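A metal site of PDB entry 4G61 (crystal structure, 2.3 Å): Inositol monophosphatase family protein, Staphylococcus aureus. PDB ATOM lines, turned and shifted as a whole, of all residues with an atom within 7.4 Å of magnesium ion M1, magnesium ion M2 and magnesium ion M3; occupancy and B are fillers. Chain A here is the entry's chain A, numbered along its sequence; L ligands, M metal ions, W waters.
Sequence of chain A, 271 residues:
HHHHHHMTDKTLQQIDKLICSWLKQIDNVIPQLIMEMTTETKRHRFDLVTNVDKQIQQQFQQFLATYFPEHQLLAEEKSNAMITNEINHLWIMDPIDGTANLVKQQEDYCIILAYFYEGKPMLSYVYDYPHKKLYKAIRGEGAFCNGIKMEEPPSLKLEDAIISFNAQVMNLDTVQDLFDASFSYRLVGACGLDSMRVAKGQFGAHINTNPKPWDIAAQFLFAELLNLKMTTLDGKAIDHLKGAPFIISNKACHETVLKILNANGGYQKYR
Magnesium ion M3 is bound by O1 of the ligand (1.9 Å), water W5 (2.1 Å), water W2 (2.1 Å), water W6 (2.2 Å), OE1 of Glu 76 (2.2 Å) and water W4 (2.4 Å). Magnesium ion M3 has six donor atoms within binding distance.
Magnesium ion M2 is bound by an oxygen (O4) of the ligand (1.9 Å), the side-chain carboxylate (OD1) of Asp 94 (2.0 Å), the backbone carbonyl oxygen (O) of Ile 96 (2.0 Å), the side-chain carboxylate (OE2) of Glu 76 (2.0 Å), water W1 (2.3 Å) and water W4 (2.3 Å).
Magnesium ion M1 is bound by O2 of the ligand, OD1 of Asp 97, OD1 of Asp 215, O4 of the ligand and OD2 of Asp 94. Magnesium ion M1 has five donor atoms within binding distance.
Water W1 lies within hydrogen-bond range of OE2 of Glu 77 (2.6 Å), OD2 of Asp 53 (2.9 Å) and N of Ile 96 (3.3 Å). Water W2 lies within hydrogen-bond range of OE2 of Glu 77 (2.5 Å), O of Leu 48 (3.0 Å) and NZ of Lys 42 (3.2 Å). Water W6 bridges the side-chain carboxylate of Asp 47 (2.7 Å) and the side-chain amino group of Lys 42 (2.9 Å). Water W3 lies within hydrogen-bond range of the indole nitrogen (NE1) of Trp 214 and the side-chain carboxylate (OD2) of Asp 215.
Of the 26 residues printed, 4 come within 4 Å of magnesium ion M2. The nearest printed residue that does not touch magnesium ion M2 is Glu 77 (4.1 Å).
N of Asp 94 is in hydrogen-bond range of O of Ile 112 (2.9 Å). The side-chain carboxylate of Asp 97 lies within hydrogen-bond range of the backbone NH of Cys 191 (3.1 Å). OG1 of Thr 99 lies close to O of Ile 96, at 3.4 Å. NZ of Lys 42 sits close to OE1 of Glu 76 (2.9 Å). The backbone NH (N) of Glu 76 lies within hydrogen-bond range of the backbone carbonyl oxygen (O) of Met 93 (3.3 Å). The backbone NH (N) of Glu 76 sits close to the side-chain amide nitrogen (NE2) of Gln 57 (3.4 Å). The backbone carbonyl oxygen (O) of Asp 215 lies within hydrogen-bond range of the side-chain sulfur (SG) of Cys 191. The side-chain amino group of Lys 42 lies within salt-bridge range of the side-chain carboxylate of Glu 77, at 3.3 Å.
Residues that only touch magnesium ion M3: Lys 42 (3.8 Å) and Leu 48 (3.8 Å). Three residues have an atom within 4 Å of magnesium ion M3: Lys 42, Leu 48 and Glu 76.
Within 4 Å of magnesium ion M1: Asp 94, Asp 97 and Asp 215. The nearest printed residue that does not touch magnesium ion M1 is Glu 76 (4.2 Å).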
ATOM      1  N   LYS A  42     -13.115  11.446 -13.938  1.00  0.00           N
ATOM      2  CA  LYS A  42     -13.286  11.697 -12.501  1.00  0.00           C
ATOM      3  C   LYS A  42     -13.948  10.491 -11.826  1.00  0.00           C
ATOM      4  O   LYS A  42     -13.278   9.471 -11.543  1.00  0.00           O
ATOM      5  CB  LYS A  42     -14.020  13.028 -12.249  1.00  0.00           C
ATOM      6  CG  LYS A  42     -13.112  14.234 -12.586  1.00  0.00           C
ATOM      7  CD  LYS A  42     -13.521  15.555 -11.882  1.00  0.00           C
ATOM      8  CE  LYS A  42     -14.762  16.159 -12.503  1.00  0.00           C
ATOM      9  NZ  LYS A  42     -15.416  17.195 -11.707  1.00  0.00           N
ATOM     10  N   ASP A  47     -17.338  10.994 -16.814  1.00  0.00           N
ATOM     11  CA  ASP A  47     -17.318  12.188 -15.972  1.00  0.00           C
ATOM     12  C   ASP A  47     -16.010  12.929 -16.266  1.00  0.00           C
ATOM     13  O   ASP A  47     -15.003  12.685 -15.614  1.00  0.00           O
ATOM     14  CB  ASP A  47     -17.359  11.793 -14.492  1.00  0.00           C
ATOM     15  CG  ASP A  47     -17.564  12.974 -13.571  1.00  0.00           C
ATOM     16  OD1 ASP A  47     -18.021  14.067 -14.049  1.00  0.00           O
ATOM     17  OD2 ASP A  47     -17.263  12.796 -12.353  1.00  0.00           O
ATOM     18  N   LEU A  48     -16.047  13.834 -17.236  1.00  0.00           N
ATOM     19  CA  LEU A  48     -14.846  14.360 -17.882  1.00  0.00           C
ATOM     20  C   LEU A  48     -14.331  15.635 -17.265  1.00  0.00           C
ATOM     21  O   LEU A  48     -15.099  16.514 -16.845  1.00  0.00           O
ATOM     22  CB  LEU A  48     -15.168  14.667 -19.333  1.00  0.00           C
ATOM     23  CG  LEU A  48     -15.026  13.603 -20.426  1.00  0.00           C
ATOM     24  CD1 LEU A  48     -15.031  12.171 -19.957  1.00  0.00           C
ATOM     25  CD2 LEU A  48     -16.003  13.860 -21.562  1.00  0.00           C
ATOM     26  N   VAL A  49     -13.011  15.766 -17.286  1.00  0.00           N
ATOM     27  CA  VAL A  49     -12.385  17.032 -17.044  1.00  0.00           C
ATOM     28  C   VAL A  49     -11.273  17.257 -18.093  1.00  0.00           C
ATOM     29  O   VAL A  49     -10.544  16.312 -18.442  1.00  0.00           O
ATOM     30  CB  VAL A  49     -11.882  17.163 -15.553  1.00  0.00           C
ATOM     31  CG1 VAL A  49     -10.745  16.164 -15.213  1.00  0.00           C
ATOM     32  CG2 VAL A  49     -11.453  18.581 -15.267  1.00  0.00           C
ATOM     33  N   ASP A  53     -10.900  23.141 -18.493  1.00  0.00           N
ATOM     34  CA  ASP A  53     -11.398  23.299 -17.116  1.00  0.00           C
ATOM     35  C   ASP A  53     -10.250  23.689 -16.189  1.00  0.00           C
ATOM     36  O   ASP A  53     -10.337  24.698 -15.545  1.00  0.00           O
ATOM     37  CB  ASP A  53     -12.081  22.033 -16.533  1.00  0.00           C
ATOM     38  CG  ASP A  53     -13.064  21.355 -17.482  1.00  0.00           C
ATOM     39  OD1 ASP A  53     -12.593  20.695 -18.450  1.00  0.00           O
ATOM     40  OD2 ASP A  53     -14.305  21.446 -17.263  1.00  0.00           O
ATOM     41  N   GLN A  57      -9.567  27.525 -14.187  1.00  0.00           N
ATOM     42  CA  GLN A  57      -9.797  27.617 -12.748  1.00  0.00           C
ATOM     43  C   GLN A  57      -8.498  28.008 -12.047  1.00  0.00           C
ATOM     44  O   GLN A  57      -8.519  28.734 -11.055  1.00  0.00           O
ATOM     45  CB  GLN A  57     -10.315  26.280 -12.183  1.00  0.00           C
ATOM     46  CG  GLN A  57     -10.505  26.295 -10.692  1.00  0.00           C
ATOM     47  CD  GLN A  57     -11.015  24.995 -10.140  1.00  0.00           C
ATOM     48  OE1 GLN A  57     -10.317  24.289  -9.420  1.00  0.00           O
ATOM     49  NE2 GLN A  57     -12.253  24.679 -10.457  1.00  0.00           N
ATOM     50  N   GLU A  76     -15.053  23.512  -8.823  1.00  0.00           N
ATOM     51  CA  GLU A  76     -15.261  22.150  -9.196  1.00  0.00           C
ATOM     52  C   GLU A  76     -14.002  21.305  -9.248  1.00  0.00           C
ATOM     53  O   GLU A  76     -14.010  20.153  -8.812  1.00  0.00           O
ATOM     54  CB  GLU A  76     -15.955  22.069 -10.557  1.00  0.00           C
ATOM     55  CG  GLU A  76     -16.334  20.617 -10.883  1.00  0.00           C
ATOM     56  CD  GLU A  76     -17.033  20.473 -12.210  1.00  0.00           C
ATOM     57  OE1 GLU A  76     -17.212  19.308 -12.651  1.00  0.00           O
ATOM     58  OE2 GLU A  76     -17.324  21.525 -12.838  1.00  0.00           O
ATOM     59  N   GLU A  77     -12.922  21.857  -9.793  1.00  0.00           N
ATOM     60  CA  GLU A  77     -11.784  21.000 -10.148  1.00  0.00           C
ATOM     61  C   GLU A  77     -10.683  21.075  -9.099  1.00  0.00           C
ATOM     62  O   GLU A  77      -9.486  21.016  -9.408  1.00  0.00           O
ATOM     63  CB  GLU A  77     -11.270  21.240 -11.577  1.00  0.00           C
ATOM     64  CG  GLU A  77     -12.346  21.406 -12.659  1.00  0.00           C
ATOM     65  CD  GLU A  77     -13.147  20.166 -12.900  1.00  0.00           C
ATOM     66  OE1 GLU A  77     -12.770  19.089 -12.360  1.00  0.00           O
ATOM     67  OE2 GLU A  77     -14.211  20.282 -13.583  1.00  0.00           O
ATOM     68  N   MET A  93     -17.021  28.871  -8.407  1.00  0.00           N
ATOM     69  CA  MET A  93     -16.723  28.747  -9.838  1.00  0.00           C
ATOM     70  C   MET A  93     -16.928  27.359 -10.443  1.00  0.00           C
ATOM     71  O   MET A  93     -16.436  26.352  -9.912  1.00  0.00           O
ATOM     72  CB  MET A  93     -15.276  29.164 -10.115  1.00  0.00           C
ATOM     73  CG  MET A  93     -14.921  29.102 -11.611  1.00  0.00           C
ATOM     74  SD  MET A  93     -13.182  29.540 -11.841  1.00  0.00           S
ATOM     75  CE  MET A  93     -13.351  30.601 -13.259  1.00  0.00           C
ATOM     76  N   ASP A  94     -17.594  27.331 -11.597  1.00  0.00           N
ATOM     77  CA  ASP A  94     -17.592  26.167 -12.466  1.00  0.00           C
ATOM     78  C   ASP A  94     -16.764  26.595 -13.690  1.00  0.00           C
ATOM     79  O   ASP A  94     -17.215  27.378 -14.509  1.00  0.00           O
ATOM     80  CB  ASP A  94     -19.024  25.813 -12.852  1.00  0.00           C
ATOM     81  CG  ASP A  94     -19.120  24.464 -13.564  1.00  0.00           C
ATOM     82  OD1 ASP A  94     -18.094  24.007 -14.104  1.00  0.00           O
ATOM     83  OD2 ASP A  94     -20.238  23.870 -13.609  1.00  0.00           O
ATOM     84  N   PRO A  95     -15.520  26.107 -13.776  1.00  0.00           N
ATOM     85  CA  PRO A  95     -14.620  26.674 -14.769  1.00  0.00           C
ATOM     86  C   PRO A  95     -15.075  26.382 -16.196  1.00  0.00           C
ATOM     87  O   PRO A  95     -14.988  27.266 -17.060  1.00  0.00           O
ATOM     88  CB  PRO A  95     -13.290  25.984 -14.478  1.00  0.00           C
ATOM     89  CG  PRO A  95     -13.624  24.828 -13.583  1.00  0.00           C
ATOM     90  CD  PRO A  95     -14.875  25.094 -12.916  1.00  0.00           C
ATOM     91  N   ILE A  96     -15.561  25.165 -16.432  1.00  0.00           N
ATOM     92  CA  ILE A  96     -16.300  24.853 -17.615  1.00  0.00           C
ATOM     93  C   ILE A  96     -17.552  24.114 -17.153  1.00  0.00           C
ATOM     94  O   ILE A  96     -17.469  23.034 -16.577  1.00  0.00           O
ATOM     95  CB  ILE A  96     -15.517  24.003 -18.638  1.00  0.00           C
ATOM     96  CG1 ILE A  96     -14.360  24.807 -19.284  1.00  0.00           C
ATOM     97  CG2 ILE A  96     -16.457  23.430 -19.695  1.00  0.00           C
ATOM     98  CD1 ILE A  96     -14.797  25.993 -20.079  1.00  0.00           C
ATOM     99  N   ASP A  97     -18.701  24.738 -17.338  1.00  0.00           N
ATOM    100  CA  ASP A  97     -19.947  24.066 -17.121  1.00  0.00           C
ATOM    101  C   ASP A  97     -20.424  23.507 -18.494  1.00  0.00           C
ATOM    102  O   ASP A  97     -20.599  24.278 -19.436  1.00  0.00           O
ATOM    103  CB  ASP A  97     -21.000  25.006 -16.534  1.00  0.00           C
ATOM    104  CG  ASP A  97     -22.267  24.271 -16.198  1.00  0.00           C
ATOM    105  OD1 ASP A  97     -22.115  23.232 -15.521  1.00  0.00           O
ATOM    106  OD2 ASP A  97     -23.401  24.675 -16.614  1.00  0.00           O
ATOM    107  N   GLY A  98     -20.608  22.180 -18.586  1.00  0.00           N
ATOM    108  CA  GLY A  98     -20.836  21.557 -19.903  1.00  0.00           C
ATOM    109  C   GLY A  98     -19.593  20.990 -20.543  1.00  0.00           C
ATOM    110  O   GLY A  98     -19.395  21.082 -21.775  1.00  0.00           O
ATOM    111  N   THR A  99     -18.755  20.359 -19.739  1.00  0.00           N
ATOM    112  CA  THR A  99     -17.497  19.810 -20.283  1.00  0.00           C
ATOM    113  C   THR A  99     -17.807  18.778 -21.395  1.00  0.00           C
ATOM    114  O   THR A  99     -17.131  18.713 -22.421  1.00  0.00           O
ATOM    115  CB  THR A  99     -16.645  19.172 -19.141  1.00  0.00           C
ATOM    116  OG1 THR A  99     -16.523  20.138 -18.085  1.00  0.00           O
ATOM    117  CG2 THR A  99     -15.301  18.822 -19.619  1.00  0.00           C
ATOM    118  N   ALA A 100     -18.850  17.970 -21.205  1.00  0.00           N
ATOM    119  CA  ALA A 100     -19.134  16.990 -22.209  1.00  0.00           C
ATOM    120  C   ALA A 100     -19.377  17.745 -23.560  1.00  0.00           C
ATOM    121  O   ALA A 100     -18.876  17.355 -24.603  1.00  0.00           O
ATOM    122  CB  ALA A 100     -20.329  16.160 -21.762  1.00  0.00           C
ATOM    123  N   CYS A 110     -20.121  26.927 -20.854  1.00  0.00           N
ATOM    124  CA  CYS A 110     -19.974  28.294 -20.378  1.00  0.00           C
ATOM    125  C   CYS A 110     -19.124  28.239 -19.133  1.00  0.00           C
ATOM    126  O   CYS A 110     -18.787  27.143 -18.641  1.00  0.00           O
ATOM    127  CB  CYS A 110     -21.319  28.859 -19.996  1.00  0.00           C
ATOM    128  SG  CYS A 110     -22.194  27.836 -18.684  1.00  0.00           S
ATOM    129  N   ILE A 112     -19.100  29.646 -15.239  1.00  0.00           N
ATOM    130  CA  ILE A 112     -19.975  30.117 -14.180  1.00  0.00           C
ATOM    131  C   ILE A 112     -19.180  30.679 -12.991  1.00  0.00           C
ATOM    132  O   ILE A 112     -18.285  30.032 -12.453  1.00  0.00           O
ATOM    133  CB  ILE A 112     -20.979  29.012 -13.764  1.00  0.00           C
ATOM    134  CG1 ILE A 112     -21.818  28.547 -14.980  1.00  0.00           C
ATOM    135  CG2 ILE A 112     -21.892  29.492 -12.575  1.00  0.00           C
ATOM    136  CD1 ILE A 112     -22.771  27.316 -14.712  1.00  0.00           C
ATOM    137  N   ALA A 190     -25.720  22.268 -20.720  1.00  0.00           N
ATOM    138  CA  ALA A 190     -25.020  22.943 -19.667  1.00  0.00           C
ATOM    139  C   ALA A 190     -26.008  23.639 -18.746  1.00  0.00           C
ATOM    140  O   ALA A 190     -26.711  24.542 -19.169  1.00  0.00           O
ATOM    141  CB  ALA A 190     -24.011  24.024 -20.248  1.00  0.00           C
ATOM    142  N   CYS A 191     -26.016  23.285 -17.473  1.00  0.00           N
ATOM    143  CA  CYS A 191     -26.938  23.891 -16.490  1.00  0.00           C
ATOM    144  C   CYS A 191     -27.012  25.435 -16.548  1.00  0.00           C
ATOM    145  O   CYS A 191     -28.096  26.017 -16.436  1.00  0.00           O
ATOM    146  CB  CYS A 191     -26.467  23.510 -15.105  1.00  0.00           C
ATOM    147  SG  CYS A 191     -27.610  23.962 -13.821  1.00  0.00           S
ATOM    148  N   GLY A 192     -25.849  26.082 -16.634  1.00  0.00           N
ATOM    149  CA  GLY A 192     -25.804  27.546 -16.697  1.00  0.00           C
ATOM    150  C   GLY A 192     -26.506  28.059 -17.928  1.00  0.00           C
ATOM    151  O   GLY A 192     -27.198  29.037 -17.869  1.00  0.00           O
ATOM    152  N   ASN A 208     -32.339  20.236 -12.657  1.00  0.00           N
ATOM    153  CA  ASN A 208     -31.135  19.368 -12.494  1.00  0.00           C
ATOM    154  C   ASN A 208     -31.326  18.691 -11.175  1.00  0.00           C
ATOM    155  O   ASN A 208     -31.379  19.367 -10.161  1.00  0.00           O
ATOM    156  CB  ASN A 208     -29.830  20.161 -12.445  1.00  0.00           C
ATOM    157  CG  ASN A 208     -28.540  19.240 -12.416  1.00  0.00           C
ATOM    158  OD1 ASN A 208     -28.524  18.145 -11.830  1.00  0.00           O
ATOM    159  ND2 ASN A 208     -27.464  19.735 -13.039  1.00  0.00           N
ATOM    160  N   LYS A 212     -24.050  20.185  -8.362  1.00  0.00           N
ATOM    161  CA  LYS A 212     -23.074  20.658  -7.390  1.00  0.00           C
ATOM    162  C   LYS A 212     -23.257  22.182  -7.160  1.00  0.00           C
ATOM    163  O   LYS A 212     -23.912  22.837  -7.971  1.00  0.00           O
ATOM    164  CB  LYS A 212     -21.685  20.281  -7.890  1.00  0.00           C
ATOM    165  CG  LYS A 212     -21.548  18.702  -8.056  1.00  0.00           C
ATOM    166  CD  LYS A 212     -21.233  18.029  -6.707  1.00  0.00           C
ATOM    167  CE  LYS A 212     -21.925  16.642  -6.521  1.00  0.00           C
ATOM    168  NZ  LYS A 212     -22.058  15.853  -7.793  1.00  0.00           N
ATOM    169  N   TRP A 214     -21.401  24.721  -7.684  1.00  0.00           N
ATOM    170  CA  TRP A 214     -20.909  25.482  -8.859  1.00  0.00           C
ATOM    171  C   TRP A 214     -21.799  25.423 -10.113  1.00  0.00           C
ATOM    172  O   TRP A 214     -21.717  26.302 -10.965  1.00  0.00           O
ATOM    173  CB  TRP A 214     -19.428  25.081  -9.182  1.00  0.00           C
ATOM    174  CG  TRP A 214     -19.206  23.559  -9.226  1.00  0.00           C
ATOM    175  CD1 TRP A 214     -19.494  22.738 -10.271  1.00  0.00           C
ATOM    176  CD2 TRP A 214     -18.690  22.695  -8.160  1.00  0.00           C
ATOM    177  NE1 TRP A 214     -19.162  21.428  -9.940  1.00  0.00           N
ATOM    178  CE2 TRP A 214     -18.667  21.370  -8.664  1.00  0.00           C
ATOM    179  CE3 TRP A 214     -18.236  22.922  -6.862  1.00  0.00           C
ATOM    180  CZ2 TRP A 214     -18.221  20.265  -7.908  1.00  0.00           C
ATOM    181  CZ3 TRP A 214     -17.803  21.825  -6.092  1.00  0.00           C
ATOM    182  CH2 TRP A 214     -17.805  20.509  -6.616  1.00  0.00           C
ATOM    183  N   ASP A 215     -22.645  24.393 -10.238  1.00  0.00           N
ATOM    184  CA  ASP A 215     -23.658  24.340 -11.328  1.00  0.00           C
ATOM    185  C   ASP A 215     -24.746  25.396 -11.214  1.00  0.00           C
ATOM    186  O   ASP A 215     -25.292  25.834 -12.221  1.00  0.00           O
ATOM    187  CB  ASP A 215     -24.292  22.960 -11.405  1.00  0.00           C
ATOM    188  CG  ASP A 215     -23.264  21.886 -11.638  1.00  0.00           C
ATOM    189  OD1 ASP A 215     -22.383  22.087 -12.484  1.00  0.00           O
ATOM    190  OD2 ASP A 215     -23.330  20.845 -10.973  1.00  0.00           O
ATOM    191  N   ILE A 216     -25.040  25.833 -10.004  1.00  0.00           N
ATOM    192  CA  ILE A 216     -26.172  26.736  -9.797  1.00  0.00           C
ATOM    193  C   ILE A 216     -25.827  28.021  -9.029  1.00  0.00           C
ATOM    194  O   ILE A 216     -26.722  28.829  -8.769  1.00  0.00           O
ATOM    195  CB  ILE A 216     -27.333  26.026  -9.068  1.00  0.00           C
ATOM    196  CG1 ILE A 216     -26.879  25.535  -7.667  1.00  0.00           C
ATOM    197  CG2 ILE A 216     -27.860  24.927  -9.935  1.00  0.00           C
ATOM    198  CD1 ILE A 216     -28.020  25.057  -6.748  1.00  0.00           C
HETATM  199  P1  LIG L   1     -19.903  20.156 -15.430  1.00  0.00           P
HETATM  200  O1  LIG L   1     -19.330  19.000 -14.588  1.00  0.00           O
HETATM  201  O2  LIG L   1     -21.422  20.263 -15.079  1.00  0.00           O
HETATM  202  O3  LIG L   1     -19.651  19.842 -16.876  1.00  0.00           O
HETATM  203  O4  LIG L   1     -19.342  21.502 -15.082  1.00  0.00           O
HETATM  204 MG    MG M   1     -21.254  21.949 -14.247  1.00  0.00          MG
HETATM  205 MG    MG M   2     -17.599  22.220 -14.736  1.00  0.00          MG
HETATM  206 MG    MG M   3     -17.640  18.241 -14.541  1.00  0.00          MG
HETATM  207  O   HOH W   1     -15.349  22.326 -14.684  1.00  0.00           O
HETATM  208  O   HOH W   2     -15.524  18.442 -14.638  1.00  0.00           O
HETATM  209  O   HOH W   3     -20.529  19.886 -12.119  1.00  0.00           O
HETATM  210  O   HOH W   4     -17.209  20.225 -15.790  1.00  0.00           O
HETATM  211  O   HOH W   5     -17.774  17.169 -16.365  1.00  0.00           O
HETATM  212  O   HOH W   6     -17.833  16.595 -13.165  1.00  0.00           O
